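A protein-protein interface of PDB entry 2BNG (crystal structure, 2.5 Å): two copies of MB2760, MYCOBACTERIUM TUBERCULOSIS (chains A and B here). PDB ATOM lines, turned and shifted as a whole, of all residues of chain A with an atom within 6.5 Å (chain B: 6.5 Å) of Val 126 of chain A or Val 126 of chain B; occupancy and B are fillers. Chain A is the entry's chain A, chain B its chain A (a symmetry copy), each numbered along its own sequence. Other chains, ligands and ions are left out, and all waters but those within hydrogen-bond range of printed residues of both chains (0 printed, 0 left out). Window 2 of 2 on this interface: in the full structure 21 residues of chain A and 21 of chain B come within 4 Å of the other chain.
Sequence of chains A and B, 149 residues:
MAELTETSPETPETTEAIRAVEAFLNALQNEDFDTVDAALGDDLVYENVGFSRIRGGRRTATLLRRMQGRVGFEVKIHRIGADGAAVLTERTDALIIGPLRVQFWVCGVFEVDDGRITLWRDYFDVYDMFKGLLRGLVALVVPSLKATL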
ATOM      1  N   PHE A  51       2.714  16.939 -22.400  1.00  0.00           N
ATOM      2  CA  PHE A  51       3.819  16.044 -22.019  1.00  0.00           C
ATOM      3  C   PHE A  51       5.021  16.671 -21.347  1.00  0.00           C
ATOM      4  O   PHE A  51       5.535  16.107 -20.400  1.00  0.00           O
ATOM      5  CB  PHE A  51       4.264  15.160 -23.191  1.00  0.00           C
ATOM      6  CG  PHE A  51       3.233  14.155 -23.577  1.00  0.00           C
ATOM      7  CD1 PHE A  51       3.208  12.885 -22.974  1.00  0.00           C
ATOM      8  CD2 PHE A  51       2.245  14.481 -24.493  1.00  0.00           C
ATOM      9  CE1 PHE A  51       2.204  11.953 -23.311  1.00  0.00           C
ATOM     10  CE2 PHE A  51       1.249  13.573 -24.833  1.00  0.00           C
ATOM     11  CZ  PHE A  51       1.230  12.310 -24.244  1.00  0.00           C
ATOM     12  N   PHE A 124       1.052  16.707 -31.081  1.00  0.00           N
ATOM     13  CA  PHE A 124       0.987  15.417 -31.723  1.00  0.00           C
ATOM     14  C   PHE A 124      -0.019  14.556 -30.974  1.00  0.00           C
ATOM     15  O   PHE A 124      -0.519  14.948 -29.918  1.00  0.00           O
ATOM     16  CB  PHE A 124       2.369  14.759 -31.705  1.00  0.00           C
ATOM     17  CG  PHE A 124       3.023  14.801 -30.368  1.00  0.00           C
ATOM     18  CD1 PHE A 124       3.939  15.808 -30.061  1.00  0.00           C
ATOM     19  CD2 PHE A 124       2.718  13.845 -29.397  1.00  0.00           C
ATOM     20  CE1 PHE A 124       4.553  15.860 -28.804  1.00  0.00           C
ATOM     21  CE2 PHE A 124       3.321  13.877 -28.149  1.00  0.00           C
ATOM     22  CZ  PHE A 124       4.238  14.890 -27.846  1.00  0.00           C
ATOM     23  N   ASP A 125      -0.260  13.357 -31.509  1.00  0.00           N
ATOM     24  CA  ASP A 125      -1.316  12.464 -31.029  1.00  0.00           C
ATOM     25  C   ASP A 125      -0.682  11.167 -30.517  1.00  0.00           C
ATOM     26  O   ASP A 125       0.085  10.547 -31.248  1.00  0.00           O
ATOM     27  CB  ASP A 125      -2.276  12.197 -32.200  1.00  0.00           C
ATOM     28  CG  ASP A 125      -3.268  11.105 -31.917  1.00  0.00           C
ATOM     29  OD1 ASP A 125      -3.731  11.009 -30.762  1.00  0.00           O
ATOM     30  OD2 ASP A 125      -3.608  10.375 -32.881  1.00  0.00           O
ATOM     31  N   VAL A 126      -1.008  10.760 -29.289  1.00  0.00           N
ATOM     32  CA  VAL A 126      -0.464   9.505 -28.740  1.00  0.00           C
ATOM     33  C   VAL A 126      -0.877   8.291 -29.569  1.00  0.00           C
ATOM     34  O   VAL A 126      -0.092   7.393 -29.765  1.00  0.00           O
ATOM     35  CB  VAL A 126      -0.817   9.253 -27.221  1.00  0.00           C
ATOM     36  CG1 VAL A 126      -0.462  10.465 -26.380  1.00  0.00           C
ATOM     37  CG2 VAL A 126      -2.263   8.927 -27.054  1.00  0.00           C
ATOM     38  N   TYR A 127      -2.104   8.256 -30.057  1.00  0.00           N
ATOM     39  CA  TYR A 127      -2.538   7.155 -30.904  1.00  0.00           C
ATOM     40  C   TYR A 127      -1.703   7.066 -32.212  1.00  0.00           C
ATOM     41  O   TYR A 127      -1.200   6.004 -32.583  1.00  0.00           O
ATOM     42  CB  TYR A 127      -4.042   7.297 -31.155  1.00  0.00           C
ATOM     43  CG  TYR A 127      -4.619   6.388 -32.208  1.00  0.00           C
ATOM     44  CD1 TYR A 127      -4.614   5.003 -32.042  1.00  0.00           C
ATOM     45  CD2 TYR A 127      -5.190   6.926 -33.377  1.00  0.00           C
ATOM     46  CE1 TYR A 127      -5.159   4.165 -33.014  1.00  0.00           C
ATOM     47  CE2 TYR A 127      -5.741   6.111 -34.356  1.00  0.00           C
ATOM     48  CZ  TYR A 127      -5.716   4.738 -34.175  1.00  0.00           C
ATOM     49  OH  TYR A 127      -6.267   3.944 -35.157  1.00  0.00           O
ATOM     50  N   ASP A 128      -1.528   8.194 -32.880  1.00  0.00           N
ATOM     51  CA  ASP A 128      -0.672   8.248 -34.037  1.00  0.00           C
ATOM     52  C   ASP A 128       0.796   7.855 -33.707  1.00  0.00           C
ATOM     53  O   ASP A 128       1.430   7.114 -34.448  1.00  0.00           O
ATOM     54  CB  ASP A 128      -0.728   9.641 -34.637  1.00  0.00           C
ATOM     55  CG  ASP A 128       0.138   9.766 -35.851  1.00  0.00           C
ATOM     56  OD1 ASP A 128      -0.231   9.171 -36.887  1.00  0.00           O
ATOM     57  OD2 ASP A 128       1.196  10.445 -35.778  1.00  0.00           O
ATOM     58  N   MET A 129       1.318   8.345 -32.590  1.00  0.00           N
ATOM     59  CA  MET A 129       2.629   7.954 -32.127  1.00  0.00           C
ATOM     60  C   MET A 129       2.717   6.489 -31.744  1.00  0.00           C
ATOM     61  O   MET A 129       3.730   5.856 -31.974  1.00  0.00           O
ATOM     62  CB  MET A 129       3.019   8.773 -30.923  1.00  0.00           C
ATOM     63  CG  MET A 129       4.523   8.785 -30.671  1.00  0.00           C
ATOM     64  SD  MET A 129       4.699  10.534 -29.832  1.00  0.00           S
ATOM     65  CE  MET A 129       4.053  11.462 -30.983  1.00  0.00           C
ATOM     66  N   PHE A 130       1.664   5.948 -31.144  1.00  0.00           N
ATOM     67  CA  PHE A 130       1.652   4.542 -30.796  1.00  0.00           C
ATOM     68  C   PHE A 130       1.738   3.713 -32.085  1.00  0.00           C
ATOM     69  O   PHE A 130       2.525   2.774 -32.167  1.00  0.00           O
ATOM     70  CB  PHE A 130       0.407   4.196 -29.950  1.00  0.00           C
ATOM     71  CG  PHE A 130       0.295   2.740 -29.605  1.00  0.00           C
ATOM     72  CD1 PHE A 130       1.147   2.168 -28.660  1.00  0.00           C
ATOM     73  CD2 PHE A 130      -0.655   1.935 -30.235  1.00  0.00           C
ATOM     74  CE1 PHE A 130       1.049   0.808 -28.338  1.00  0.00           C
ATOM     75  CE2 PHE A 130      -0.775   0.569 -29.923  1.00  0.00           C
ATOM     76  CZ  PHE A 130       0.081   0.004 -28.977  1.00  0.00           C
ATOM     77  N   LYS A 131       0.942   4.082 -33.089  1.00  0.00           N
ATOM     78  CA  LYS A 131       0.947   3.386 -34.383  1.00  0.00           C
ATOM     79  C   LYS A 131       2.316   3.477 -35.041  1.00  0.00           C
ATOM     80  O   LYS A 131       2.784   2.516 -35.647  1.00  0.00           O
ATOM     81  CB  LYS A 131      -0.115   3.959 -35.334  1.00  0.00           C
ATOM     82  CG  LYS A 131      -1.558   3.549 -35.028  1.00  0.00           C
ATOM     83  CD  LYS A 131      -2.524   4.037 -36.121  1.00  0.00           C
ATOM     84  CE  LYS A 131      -2.679   5.574 -36.094  1.00  0.00           C
ATOM     85  NZ  LYS A 131      -3.506   6.128 -37.199  1.00  0.00           N
ATOM     86  N   PHE B  51      -8.908   9.469 -38.240  1.00  0.00           N
ATOM     87  CA  PHE B  51     -10.270   9.086 -37.830  1.00  0.00           C
ATOM     88  C   PHE B  51     -11.344   9.096 -38.897  1.00  0.00           C
ATOM     89  O   PHE B  51     -12.154   8.188 -38.933  1.00  0.00           O
ATOM     90  CB  PHE B  51     -10.735   9.874 -36.599  1.00  0.00           C
ATOM     91  CG  PHE B  51      -9.978   9.510 -35.366  1.00  0.00           C
ATOM     92  CD1 PHE B  51     -10.419   8.465 -34.536  1.00  0.00           C
ATOM     93  CD2 PHE B  51      -8.794  10.161 -35.054  1.00  0.00           C
ATOM     94  CE1 PHE B  51      -9.675   8.097 -33.395  1.00  0.00           C
ATOM     95  CE2 PHE B  51      -8.052   9.808 -33.934  1.00  0.00           C
ATOM     96  CZ  PHE B  51      -8.492   8.778 -33.104  1.00  0.00           C
ATOM     97  N   PHE B 124      -5.891  16.456 -33.740  1.00  0.00           N
ATOM     98  CA  PHE B 124      -6.082  16.473 -32.311  1.00  0.00           C
ATOM     99  C   PHE B 124      -5.506  15.188 -31.731  1.00  0.00           C
ATOM    100  O   PHE B 124      -5.108  14.287 -32.472  1.00  0.00           O
ATOM    101  CB  PHE B 124      -7.574  16.581 -31.988  1.00  0.00           C
ATOM    102  CG  PHE B 124      -8.412  15.619 -32.755  1.00  0.00           C
ATOM    103  CD1 PHE B 124      -9.046  16.019 -33.933  1.00  0.00           C
ATOM    104  CD2 PHE B 124      -8.563  14.301 -32.319  1.00  0.00           C
ATOM    105  CE1 PHE B 124      -9.830  15.120 -34.666  1.00  0.00           C
ATOM    106  CE2 PHE B 124      -9.341  13.399 -33.029  1.00  0.00           C
ATOM    107  CZ  PHE B 124      -9.974  13.805 -34.210  1.00  0.00           C
ATOM    108  N   ASP B 125      -5.523  15.101 -30.400  1.00  0.00           N
ATOM    109  CA  ASP B 125      -4.863  14.023 -29.660  1.00  0.00           C
ATOM    110  C   ASP B 125      -5.916  13.232 -28.879  1.00  0.00           C
ATOM    111  O   ASP B 125      -6.686  13.832 -28.136  1.00  0.00           O
ATOM    112  CB  ASP B 125      -3.829  14.662 -28.720  1.00  0.00           C
ATOM    113  CG  ASP B 125      -3.250  13.694 -27.728  1.00  0.00           C
ATOM    114  OD1 ASP B 125      -3.042  12.521 -28.097  1.00  0.00           O
ATOM    115  OD2 ASP B 125      -2.967  14.140 -26.588  1.00  0.00           O
ATOM    116  N   VAL B 126      -5.937  11.906 -29.036  1.00  0.00           N
ATOM    117  CA  VAL B 126      -6.901  11.075 -28.293  1.00  0.00           C
ATOM    118  C   VAL B 126      -6.710  11.187 -26.783  1.00  0.00           C
ATOM    119  O   VAL B 126      -7.669  11.214 -26.048  1.00  0.00           O
ATOM    120  CB  VAL B 126      -6.906   9.551 -28.713  1.00  0.00           C
ATOM    121  CG1 VAL B 126      -7.044   9.412 -30.218  1.00  0.00           C
ATOM    122  CG2 VAL B 126      -5.662   8.867 -28.254  1.00  0.00           C
ATOM    123  N   TYR B 127      -5.476  11.252 -26.312  1.00  0.00           N
ATOM    124  CA  TYR B 127      -5.230  11.420 -24.888  1.00  0.00           C
ATOM    125  C   TYR B 127      -5.814  12.756 -24.353  1.00  0.00           C
ATOM    126  O   TYR B 127      -6.524  12.791 -23.345  1.00  0.00           O
ATOM    127  CB  TYR B 127      -3.726  11.271 -24.633  1.00  0.00           C
ATOM    128  CG  TYR B 127      -3.255  11.656 -23.255  1.00  0.00           C
ATOM    129  CD1 TYR B 127      -3.680  10.951 -22.129  1.00  0.00           C
ATOM    130  CD2 TYR B 127      -2.360  12.729 -23.084  1.00  0.00           C
ATOM    131  CE1 TYR B 127      -3.233  11.304 -20.856  1.00  0.00           C
ATOM    132  CE2 TYR B 127      -1.900  13.095 -21.826  1.00  0.00           C
ATOM    133  CZ  TYR B 127      -2.343  12.388 -20.720  1.00  0.00           C
ATOM    134  OH  TYR B 127      -1.875  12.765 -19.480  1.00  0.00           O
ATOM    135  N   ASP B 128      -5.545  13.844 -25.055  1.00  0.00           N
ATOM    136  CA  ASP B 128      -6.134  15.113 -24.718  1.00  0.00           C
ATOM    137  C   ASP B 128      -7.688  15.081 -24.784  1.00  0.00           C
ATOM    138  O   ASP B 128      -8.365  15.605 -23.908  1.00  0.00           O
ATOM    139  CB  ASP B 128      -5.584  16.183 -25.642  1.00  0.00           C
ATOM    140  CG  ASP B 128      -6.155  17.534 -25.341  1.00  0.00           C
ATOM    141  OD1 ASP B 128      -5.793  18.090 -24.281  1.00  0.00           O
ATOM    142  OD2 ASP B 128      -6.972  18.044 -26.150  1.00  0.00           O
ATOM    143  N   MET B 129      -8.237  14.455 -25.817  1.00  0.00           N
ATOM    144  CA  MET B 129      -9.666  14.264 -25.920  1.00  0.00           C
ATOM    145  C   MET B 129     -10.227  13.363 -24.838  1.00  0.00           C
ATOM    146  O   MET B 129     -11.322  13.591 -24.358  1.00  0.00           O
ATOM    147  CB  MET B 129     -10.012  13.659 -27.256  1.00  0.00           C
ATOM    148  CG  MET B 129     -11.471  13.869 -27.646  1.00  0.00           C
ATOM    149  SD  MET B 129     -11.290  13.898 -29.585  1.00  0.00           S
ATOM    150  CE  MET B 129     -10.218  15.092 -29.748  1.00  0.00           C
ATOM    151  N   PHE B 130      -9.492  12.324 -24.461  1.00  0.00           N
ATOM    152  CA  PHE B 130      -9.939  11.449 -23.397  1.00  0.00           C
ATOM    153  C   PHE B 130     -10.029  12.258 -22.096  1.00  0.00           C
ATOM    154  O   PHE B 130     -11.021  12.171 -21.378  1.00  0.00           O
ATOM    155  CB  PHE B 130      -9.010  10.222 -23.269  1.00  0.00           C
ATOM    156  CG  PHE B 130      -9.374   9.301 -22.143  1.00  0.00           C
ATOM    157  CD1 PHE B 130     -10.505   8.487 -22.230  1.00  0.00           C
ATOM    158  CD2 PHE B 130      -8.596   9.254 -20.985  1.00  0.00           C
ATOM    159  CE1 PHE B 130     -10.852   7.629 -21.179  1.00  0.00           C
ATOM    160  CE2 PHE B 130      -8.922   8.395 -19.920  1.00  0.00           C
ATOM    161  CZ  PHE B 130     -10.055   7.585 -20.016  1.00  0.00           C
ATOM    162  N   LYS B 131      -8.998  13.057 -21.814  1.00  0.00           N
ATOM    163  CA  LYS B 131      -8.973  13.901 -20.612  1.00  0.00           C
ATOM    164  C   LYS B 131     -10.125  14.896 -20.626  1.00  0.00           C
ATOM    165  O   LYS B 131     -10.730  15.166 -19.592  1.00  0.00           O
ATOM    166  CB  LYS B 131      -7.643  14.661 -20.486  1.00  0.00           C
ATOM    167  CG  LYS B 131      -6.451  13.821 -20.018  1.00  0.00           C
ATOM    168  CD  LYS B 131      -5.211  14.698 -19.770  1.00  0.00           C
ATOM    169  CE  LYS B 131      -4.637  15.252 -21.091  1.00  0.00           C
ATOM    170  NZ  LYS B 131      -3.507  16.204 -20.919  1.00  0.00           N
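N of Val 126 of chain B is in hydrogen-bond range of OD1 of Asp 125 of chain A. N of Val 126 of chain A is in hydrogen-bond range of OD1 of Asp 125 of chain B, at 2.9 Å. The side-chain carboxylate of Asp 125 of chain A lies close to the side-chain carboxylate of Asp 125 of chain B, at 3.1 Å.
The side-chain carboxylate (OD1) of Asp 125 of chain A sits close to the backbone NH (N) of Tyr 127 of chain A, at 3.3 Å. OD2 of Asp 125 of chain A is in hydrogen-bond range of N of Asp 128 of chain A. The backbone NH of Tyr 127 of chain B lies close to the side-chain carboxylate of Asp 125 of chain B (3.3 Å). OD2 of Asp 125 of chain B sits at hydrogen-bond distance from N of Asp 128 of chain B (3.0 Å).
Among the printed residues, merely in contact across the chains: Phe 51 of chain A with Tyr 127 of chain B (3.8 Å), Phe 124 of chain A with Asp 125 of chain B (3.5 Å), Asp 125 of chain A with Phe 124 of chain B (3.5 Å), Val 126 of chain A with Val 126 of chain B (3.6 Å), Val 126 of chain A with Tyr 127 of chain B (3.7 Å), Tyr 127 of chain A with Phe 51 of chain B (3.8 Å) and Tyr 127 of chain A with Val 126 of chain B (3.7 Å).
Phe 51 of chain A touches Tyr 127 of chain B, and with the chains exchanged Tyr 127 of chain A touches Phe 51 of chain B. Asp 125 of chain B touches its own counterpart, Asp 125 of chain A. Val 126 of chain A touches its own counterpart, Val 126 of chain B. Val 126 of chain A touches Tyr 127 of chain B, and with the chains exchanged Tyr 127 of chain A touches Val 126 of chain B.
Of chain B, only Asp 125, Val 126 and Tyr 127 come within 4 Å of Val 126 of chain A. Of the printed residues of chain A, Val 126 of chain B touches Asp 125 (2.9 Å), Val 126 (3.6 Å) and Tyr 127 (3.7 Å). Of the printed residues of chain B, Asp 125 of chain A touches Phe 124 (3.5 Å), Asp 125 (3.1 Å) and Val 126 (2.9 Å). Printed residues of chain B within 4 Å of Phe 124 of chain A: Asp 125. Of the printed residues of chain B, Phe 51 of chain A touches Tyr 127 (3.8 Å). Printed residues of chain B within 4 Å of Tyr 127 of chain A: Phe 51 and Val 126. Printed residues of chain A within 4 Å of Phe 124 of chain B: Asp 125 (3.5 Å). Asp 128 of chain A touches none of the printed residues of chain B. Lys 131 of chain B touches none of the printed residues of chain A. The nearest residue of chain B that does not touch Val 126 of chain A is Asp 128 of chain B (6.2 Å). The nearest residue of chain A that does not touch Val 126 of chain B is Asp 128 of chain A (6.2 Å).
Hydrophobic or aromatic side chains of chain B that line the printed part of chain A: Phe 51, Val 126 and Tyr 127. Of the 9 printed residues of chain A, 5 touch a printed residue of chain B. Among the printed residues, no Asp or Glu carboxylate lies within 4 Å of a Lys or Arg side-chain nitrogen of the other chain.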
